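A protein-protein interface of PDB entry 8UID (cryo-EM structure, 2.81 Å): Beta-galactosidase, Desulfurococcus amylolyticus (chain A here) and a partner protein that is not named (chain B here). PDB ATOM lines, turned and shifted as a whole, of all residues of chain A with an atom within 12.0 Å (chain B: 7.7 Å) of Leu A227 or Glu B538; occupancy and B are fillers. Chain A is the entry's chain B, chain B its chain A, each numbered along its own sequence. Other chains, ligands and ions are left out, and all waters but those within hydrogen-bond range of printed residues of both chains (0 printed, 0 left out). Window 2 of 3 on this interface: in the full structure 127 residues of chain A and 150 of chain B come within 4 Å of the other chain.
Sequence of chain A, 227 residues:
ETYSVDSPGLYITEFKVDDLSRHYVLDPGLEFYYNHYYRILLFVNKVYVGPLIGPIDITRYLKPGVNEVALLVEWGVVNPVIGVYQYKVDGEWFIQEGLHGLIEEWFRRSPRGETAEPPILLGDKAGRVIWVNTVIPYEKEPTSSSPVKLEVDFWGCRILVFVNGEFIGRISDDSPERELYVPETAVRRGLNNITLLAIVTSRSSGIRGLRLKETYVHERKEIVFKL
The backbone NH (N) of Phe A225 sits at hydrogen-bond distance from the backbone carbonyl oxygen (O) of Val B515, at 2.8 Å.
The backbone carbonyl oxygen of Lys A226 sits at hydrogen-bond distance from the backbone NH of Glu B538, at 2.8 Å.
N of Lys A226 is in hydrogen-bond range of O of Ala B539.
N of Ile B537 lies within hydrogen-bond range of OH of Tyr B557, at 3.2 Å.
O of Ile B540 sits at hydrogen-bond distance from N of Leu B547 (2.9 Å).
Among the printed residues, pairs that only touch across the chains: Val A224 with Lys B514 (3.5 Å), Val A224 with Val B515 (3.4 Å), Val A224 with Ala B539 (3.99 Å), Val A224 with Ile B540 (3.3 Å), Phe A225 with Lys B514 (3.3 Å), Phe A225 with Ala B539 (3.4 Å), Phe A225 with Ile B540 (3.6 Å), Lys A226 with Glu B536 (3.9998 Å), Lys A226 with Ile B537 (3.5 Å), Leu A227 with Gly B513 (3.9 Å), Leu A227 with Glu B536 (3.0 Å), Leu A227 with Ile B537 (3.7 Å) and Leu A227 with Glu B538 (3.9 Å).
Leu A227 touches just these residues of chain B: Gly B513, Glu B536, Ile B537 and Glu B538.
Ile B510 touches none of the printed residues of chain A.
Of the printed residues of chain A, Gly B513 touches Leu A227 (3.9 Å).
No residue of chain A comes within 4 Å of Arg B535.
Of the printed residues of chain A, Glu B536 touches Lys A226 and Leu A227.
Of chain A, only Lys A226 (2.8 Å) and Leu A227 (3.9 Å) come within 4 Å of Glu B538.
Of the printed residues of chain A, Ala B539 touches Val A224 (3.99 Å), Phe A225 (3.4 Å) and Lys A226 (3.0 Å).
No residue of chain A comes within 4 Å of Leu B549.
The nearest residue of chain B that does not touch Leu A227 is Arg B535 (4.1 Å).
The nearest printed residue of chain B that does not touch Val A224 is Ile B537 (6.4 Å).
Of the 18 printed residues of chain B, 8 touch a printed residue of chain A.
Hydrophobic or aromatic side chains of chain B within 4 Å of the printed part of chain A: Ile B537 and Ile B540.
Of the 5 printed residues of chain A, 4 touch a printed residue of chain B.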
ATOM      1  N   ILE A 223     -16.505 -21.277  10.359  1.00  0.00           N
ATOM      2  CA  ILE A 223     -17.878 -21.185  10.878  1.00  0.00           C
ATOM      3  C   ILE A 223     -18.028 -19.860  11.615  1.00  0.00           C
ATOM      4  O   ILE A 223     -17.169 -19.474  12.402  1.00  0.00           O
ATOM      5  CB  ILE A 223     -18.251 -22.393  11.763  1.00  0.00           C
ATOM      6  CG1 ILE A 223     -18.201 -23.693  10.936  1.00  0.00           C
ATOM      7  CG2 ILE A 223     -19.639 -22.215  12.403  1.00  0.00           C
ATOM      8  CD1 ILE A 223     -18.602 -24.965  11.695  1.00  0.00           C
ATOM      9  N   VAL A 224     -19.109 -19.141  11.350  1.00  0.00           N
ATOM     10  CA  VAL A 224     -19.291 -17.740  11.732  1.00  0.00           C
ATOM     11  C   VAL A 224     -20.633 -17.567  12.424  1.00  0.00           C
ATOM     12  O   VAL A 224     -21.635 -18.053  11.916  1.00  0.00           O
ATOM     13  CB  VAL A 224     -19.208 -16.836  10.489  1.00  0.00           C
ATOM     14  CG1 VAL A 224     -19.332 -15.362  10.869  1.00  0.00           C
ATOM     15  CG2 VAL A 224     -17.909 -17.046   9.703  1.00  0.00           C
ATOM     16  N   PHE A 225     -20.680 -16.846  13.539  1.00  0.00           N
ATOM     17  CA  PHE A 225     -21.888 -16.568  14.313  1.00  0.00           C
ATOM     18  C   PHE A 225     -22.112 -15.059  14.371  1.00  0.00           C
ATOM     19  O   PHE A 225     -21.315 -14.338  14.971  1.00  0.00           O
ATOM     20  CB  PHE A 225     -21.767 -17.130  15.742  1.00  0.00           C
ATOM     21  CG  PHE A 225     -21.345 -18.577  15.882  1.00  0.00           C
ATOM     22  CD1 PHE A 225     -20.018 -18.950  15.614  1.00  0.00           C
ATOM     23  CD2 PHE A 225     -22.261 -19.555  16.300  1.00  0.00           C
ATOM     24  CE1 PHE A 225     -19.637 -20.294  15.654  1.00  0.00           C
ATOM     25  CE2 PHE A 225     -21.879 -20.905  16.334  1.00  0.00           C
ATOM     26  CZ  PHE A 225     -20.575 -21.278  15.991  1.00  0.00           C
ATOM     27  N   LYS A 226     -23.208 -14.561  13.799  1.00  0.00           N
ATOM     28  CA  LYS A 226     -23.658 -13.172  14.006  1.00  0.00           C
ATOM     29  C   LYS A 226     -24.334 -13.080  15.372  1.00  0.00           C
ATOM     30  O   LYS A 226     -25.051 -14.004  15.737  1.00  0.00           O
ATOM     31  CB  LYS A 226     -24.560 -12.752  12.834  1.00  0.00           C
ATOM     32  CG  LYS A 226     -24.930 -11.259  12.875  1.00  0.00           C
ATOM     33  CD  LYS A 226     -25.506 -10.737  11.548  1.00  0.00           C
ATOM     34  CE  LYS A 226     -26.787 -11.454  11.106  1.00  0.00           C
ATOM     35  NZ  LYS A 226     -27.364 -10.830   9.890  1.00  0.00           N
ATOM     36  N   LEU A 227     -24.130 -12.015  16.144  1.00  0.00           N
ATOM     37  CA  LEU A 227     -24.634 -11.908  17.527  1.00  0.00           C
ATOM     38  C   LEU A 227     -25.892 -11.034  17.630  1.00  0.00           C
ATOM     39  O   LEU A 227     -25.905  -9.894  17.160  1.00  0.00           O
ATOM     40  CB  LEU A 227     -23.529 -11.423  18.485  1.00  0.00           C
ATOM     41  CG  LEU A 227     -22.245 -12.271  18.539  1.00  0.00           C
ATOM     42  CD1 LEU A 227     -21.409 -11.816  19.731  1.00  0.00           C
ATOM     43  CD2 LEU A 227     -22.505 -13.766  18.702  1.00  0.00           C
ATOM     44  N   LEU B 496     -19.468 -20.374  25.082  1.00  0.00           N
ATOM     45  CA  LEU B 496     -19.816 -20.976  23.789  1.00  0.00           C
ATOM     46  C   LEU B 496     -19.428 -22.463  23.739  1.00  0.00           C
ATOM     47  O   LEU B 496     -18.260 -22.803  23.583  1.00  0.00           O
ATOM     48  CB  LEU B 496     -19.154 -20.155  22.663  1.00  0.00           C
ATOM     49  CG  LEU B 496     -19.639 -20.422  21.234  1.00  0.00           C
ATOM     50  CD1 LEU B 496     -21.146 -20.254  21.073  1.00  0.00           C
ATOM     51  CD2 LEU B 496     -18.994 -19.408  20.295  1.00  0.00           C
ATOM     52  N   ILE B 510     -13.208 -14.575  18.951  1.00  0.00           N
ATOM     53  CA  ILE B 510     -14.343 -14.177  19.796  1.00  0.00           C
ATOM     54  C   ILE B 510     -14.491 -12.644  19.738  1.00  0.00           C
ATOM     55  O   ILE B 510     -14.144 -11.912  20.664  1.00  0.00           O
ATOM     56  CB  ILE B 510     -14.183 -14.731  21.237  1.00  0.00           C
ATOM     57  CG1 ILE B 510     -13.984 -16.262  21.317  1.00  0.00           C
ATOM     58  CG2 ILE B 510     -15.384 -14.352  22.121  1.00  0.00           C
ATOM     59  CD1 ILE B 510     -15.182 -17.118  20.879  1.00  0.00           C
ATOM     60  N   ASP B 511     -14.922 -12.136  18.591  1.00  0.00           N
ATOM     61  CA  ASP B 511     -15.112 -10.702  18.355  1.00  0.00           C
ATOM     62  C   ASP B 511     -16.362 -10.153  19.065  1.00  0.00           C
ATOM     63  O   ASP B 511     -17.325 -10.873  19.330  1.00  0.00           O
ATOM     64  CB  ASP B 511     -15.195 -10.424  16.847  1.00  0.00           C
ATOM     65  CG  ASP B 511     -13.933 -10.772  16.050  1.00  0.00           C
ATOM     66  OD1 ASP B 511     -12.881 -11.089  16.646  1.00  0.00           O
ATOM     67  OD2 ASP B 511     -13.967 -10.637  14.807  1.00  0.00           O
ATOM     68  N   GLU B 512     -16.375  -8.847  19.339  1.00  0.00           N
ATOM     69  CA  GLU B 512     -17.516  -8.091  19.872  1.00  0.00           C
ATOM     70  C   GLU B 512     -18.612  -7.877  18.801  1.00  0.00           C
ATOM     71  O   GLU B 512     -18.932  -6.753  18.412  1.00  0.00           O
ATOM     72  CB  GLU B 512     -17.022  -6.762  20.479  1.00  0.00           C
ATOM     73  CG  GLU B 512     -16.070  -6.930  21.679  1.00  0.00           C
ATOM     74  CD  GLU B 512     -14.619  -7.334  21.341  1.00  0.00           C
ATOM     75  OE1 GLU B 512     -14.185  -7.223  20.170  1.00  0.00           O
ATOM     76  OE2 GLU B 512     -13.890  -7.745  22.271  1.00  0.00           O
ATOM     77  N   GLY B 513     -19.157  -8.982  18.289  1.00  0.00           N
ATOM     78  CA  GLY B 513     -19.982  -9.059  17.078  1.00  0.00           C
ATOM     79  C   GLY B 513     -19.245  -9.800  15.957  1.00  0.00           C
ATOM     80  O   GLY B 513     -18.092  -9.489  15.668  1.00  0.00           O
ATOM     81  N   LYS B 514     -19.904 -10.783  15.328  1.00  0.00           N
ATOM     82  CA  LYS B 514     -19.332 -11.737  14.352  1.00  0.00           C
ATOM     83  C   LYS B 514     -18.195 -12.597  14.929  1.00  0.00           C
ATOM     84  O   LYS B 514     -17.037 -12.463  14.555  1.00  0.00           O
ATOM     85  CB  LYS B 514     -18.983 -11.021  13.032  1.00  0.00           C
ATOM     86  CG  LYS B 514     -18.795 -12.016  11.873  1.00  0.00           C
ATOM     87  CD  LYS B 514     -18.358 -11.333  10.570  1.00  0.00           C
ATOM     88  CE  LYS B 514     -19.428 -10.420   9.951  1.00  0.00           C
ATOM     89  NZ  LYS B 514     -20.466 -11.172   9.200  1.00  0.00           N
ATOM     90  N   VAL B 515     -18.540 -13.513  15.832  1.00  0.00           N
ATOM     91  CA  VAL B 515     -17.638 -14.574  16.316  1.00  0.00           C
ATOM     92  C   VAL B 515     -17.290 -15.535  15.177  1.00  0.00           C
ATOM     93  O   VAL B 515     -18.160 -15.880  14.385  1.00  0.00           O
ATOM     94  CB  VAL B 515     -18.284 -15.348  17.481  1.00  0.00           C
ATOM     95  CG1 VAL B 515     -17.513 -16.614  17.862  1.00  0.00           C
ATOM     96  CG2 VAL B 515     -18.383 -14.455  18.716  1.00  0.00           C
ATOM     97  N   THR B 533     -24.951 -21.289  24.755  1.00  0.00           N
ATOM     98  CA  THR B 533     -24.326 -19.972  24.963  1.00  0.00           C
ATOM     99  C   THR B 533     -25.308 -18.936  25.504  1.00  0.00           C
ATOM    100  O   THR B 533     -26.493 -18.985  25.195  1.00  0.00           O
ATOM    101  CB  THR B 533     -23.742 -19.459  23.639  1.00  0.00           C
ATOM    102  OG1 THR B 533     -23.172 -18.193  23.814  1.00  0.00           O
ATOM    103  CG2 THR B 533     -24.747 -19.346  22.495  1.00  0.00           C
ATOM    104  N   ARG B 535     -24.795 -15.781  24.549  1.00  0.00           N
ATOM    105  CA  ARG B 535     -24.798 -14.847  23.420  1.00  0.00           C
ATOM    106  C   ARG B 535     -26.067 -15.016  22.596  1.00  0.00           C
ATOM    107  O   ARG B 535     -26.494 -16.134  22.322  1.00  0.00           O
ATOM    108  CB  ARG B 535     -23.573 -15.075  22.528  1.00  0.00           C
ATOM    109  CG  ARG B 535     -22.246 -14.790  23.238  1.00  0.00           C
ATOM    110  CD  ARG B 535     -21.076 -15.056  22.287  1.00  0.00           C
ATOM    111  NE  ARG B 535     -19.813 -14.581  22.868  1.00  0.00           N
ATOM    112  CZ  ARG B 535     -18.955 -15.273  23.585  1.00  0.00           C
ATOM    113  NH1 ARG B 535     -17.909 -14.714  24.101  1.00  0.00           N
ATOM    114  NH2 ARG B 535     -19.084 -16.533  23.852  1.00  0.00           N
ATOM    115  N   GLU B 536     -26.657 -13.915  22.155  1.00  0.00           N
ATOM    116  CA  GLU B 536     -27.825 -13.963  21.280  1.00  0.00           C
ATOM    117  C   GLU B 536     -27.388 -14.219  19.833  1.00  0.00           C
ATOM    118  O   GLU B 536     -27.138 -13.287  19.073  1.00  0.00           O
ATOM    119  CB  GLU B 536     -28.662 -12.690  21.456  1.00  0.00           C
ATOM    120  CG  GLU B 536     -29.973 -12.776  20.662  1.00  0.00           C
ATOM    121  CD  GLU B 536     -31.050 -11.825  21.206  1.00  0.00           C
ATOM    122  OE1 GLU B 536     -30.765 -10.627  21.423  1.00  0.00           O
ATOM    123  OE2 GLU B 536     -32.200 -12.270  21.408  1.00  0.00           O
ATOM    124  N   ILE B 537     -27.244 -15.490  19.455  1.00  0.00           N
ATOM    125  CA  ILE B 537     -26.858 -15.880  18.099  1.00  0.00           C
ATOM    126  C   ILE B 537     -27.990 -15.525  17.122  1.00  0.00           C
ATOM    127  O   ILE B 537     -29.086 -16.075  17.183  1.00  0.00           O
ATOM    128  CB  ILE B 537     -26.476 -17.374  18.035  1.00  0.00           C
ATOM    129  CG1 ILE B 537     -25.477 -17.824  19.121  1.00  0.00           C
ATOM    130  CG2 ILE B 537     -25.930 -17.708  16.642  1.00  0.00           C
ATOM    131  CD1 ILE B 537     -24.189 -17.002  19.204  1.00  0.00           C
ATOM    132  N   GLU B 538     -27.731 -14.577  16.228  1.00  0.00           N
ATOM    133  CA  GLU B 538     -28.676 -14.046  15.242  1.00  0.00           C
ATOM    134  C   GLU B 538     -28.655 -14.859  13.937  1.00  0.00           C
ATOM    135  O   GLU B 538     -29.686 -15.027  13.288  1.00  0.00           O
ATOM    136  CB  GLU B 538     -28.308 -12.571  14.995  1.00  0.00           C
ATOM    137  CG  GLU B 538     -29.245 -11.778  14.069  1.00  0.00           C
ATOM    138  CD  GLU B 538     -30.605 -11.395  14.685  1.00  0.00           C
ATOM    139  OE1 GLU B 538     -30.879 -11.709  15.864  1.00  0.00           O
ATOM    140  OE2 GLU B 538     -31.410 -10.740  13.987  1.00  0.00           O
ATOM    141  N   ALA B 539     -27.484 -15.385  13.566  1.00  0.00           N
ATOM    142  CA  ALA B 539     -27.290 -16.282  12.435  1.00  0.00           C
ATOM    143  C   ALA B 539     -26.057 -17.166  12.651  1.00  0.00           C
ATOM    144  O   ALA B 539     -25.126 -16.767  13.345  1.00  0.00           O
ATOM    145  CB  ALA B 539     -27.132 -15.452  11.159  1.00  0.00           C
ATOM    146  N   ILE B 540     -26.010 -18.324  11.999  1.00  0.00           N
ATOM    147  CA  ILE B 540     -24.801 -19.139  11.872  1.00  0.00           C
ATOM    148  C   ILE B 540     -24.553 -19.355  10.385  1.00  0.00           C
ATOM    149  O   ILE B 540     -25.465 -19.675   9.631  1.00  0.00           O
ATOM    150  CB  ILE B 540     -24.886 -20.473  12.651  1.00  0.00           C
ATOM    151  CG1 ILE B 540     -25.124 -20.214  14.154  1.00  0.00           C
ATOM    152  CG2 ILE B 540     -23.601 -21.302  12.471  1.00  0.00           C
ATOM    153  CD1 ILE B 540     -25.533 -21.450  14.962  1.00  0.00           C
ATOM    154  N   ASP B 546     -25.247 -19.785   4.486  1.00  0.00           N
ATOM    155  CA  ASP B 546     -26.119 -19.552   5.638  1.00  0.00           C
ATOM    156  C   ASP B 546     -26.712 -20.874   6.161  1.00  0.00           C
ATOM    157  O   ASP B 546     -27.269 -21.645   5.379  1.00  0.00           O
ATOM    158  CB  ASP B 546     -27.232 -18.590   5.210  1.00  0.00           C
ATOM    159  CG  ASP B 546     -28.140 -18.211   6.376  1.00  0.00           C
ATOM    160  OD1 ASP B 546     -27.610 -17.722   7.394  1.00  0.00           O
ATOM    161  OD2 ASP B 546     -29.374 -18.373   6.256  1.00  0.00           O
ATOM    162  N   LEU B 547     -26.636 -21.139   7.467  1.00  0.00           N
ATOM    163  CA  LEU B 547     -27.250 -22.306   8.104  1.00  0.00           C
ATOM    164  C   LEU B 547     -28.553 -21.915   8.817  1.00  0.00           C
ATOM    165  O   LEU B 547     -28.670 -20.840   9.397  1.00  0.00           O
ATOM    166  CB  LEU B 547     -26.273 -22.998   9.067  1.00  0.00           C
ATOM    167  CG  LEU B 547     -24.868 -23.328   8.531  1.00  0.00           C
ATOM    168  CD1 LEU B 547     -24.117 -24.154   9.576  1.00  0.00           C
ATOM    169  CD2 LEU B 547     -24.904 -24.146   7.240  1.00  0.00           C
ATOM    170  N   LEU B 549     -31.370 -21.883  11.725  1.00  0.00           N
ATOM    171  CA  LEU B 549     -31.387 -21.903  13.195  1.00  0.00           C
ATOM    172  C   LEU B 549     -32.755 -22.317  13.749  1.00  0.00           C
ATOM    173  O   LEU B 549     -33.790 -21.821  13.304  1.00  0.00           O
ATOM    174  CB  LEU B 549     -31.033 -20.517  13.766  1.00  0.00           C
ATOM    175  CG  LEU B 549     -29.549 -20.343  14.086  1.00  0.00           C
ATOM    176  CD1 LEU B 549     -28.695 -20.451  12.834  1.00  0.00           C
ATOM    177  CD2 LEU B 549     -29.318 -18.983  14.735  1.00  0.00           C
ATOM    178  N   TYR B 557     -29.193 -23.199  20.673  1.00  0.00           N
ATOM    179  CA  TYR B 557     -29.492 -23.112  19.246  1.00  0.00           C
ATOM    180  C   TYR B 557     -29.124 -24.418  18.538  1.00  0.00           C
ATOM    181  O   TYR B 557     -27.979 -24.844  18.591  1.00  0.00           O
ATOM    182  CB  TYR B 557     -28.729 -21.935  18.626  1.00  0.00           C
ATOM    183  CG  TYR B 557     -29.035 -20.582  19.230  1.00  0.00           C
ATOM    184  CD1 TYR B 557     -28.326 -20.118  20.355  1.00  0.00           C
ATOM    185  CD2 TYR B 557     -30.021 -19.771  18.646  1.00  0.00           C
ATOM    186  CE1 TYR B 557     -28.608 -18.851  20.897  1.00  0.00           C
ATOM    187  CE2 TYR B 557     -30.292 -18.495  19.169  1.00  0.00           C
ATOM    188  CZ  TYR B 557     -29.587 -18.039  20.299  1.00  0.00           C
ATOM    189  OH  TYR B 557     -29.842 -16.803  20.795  1.00  0.00           O
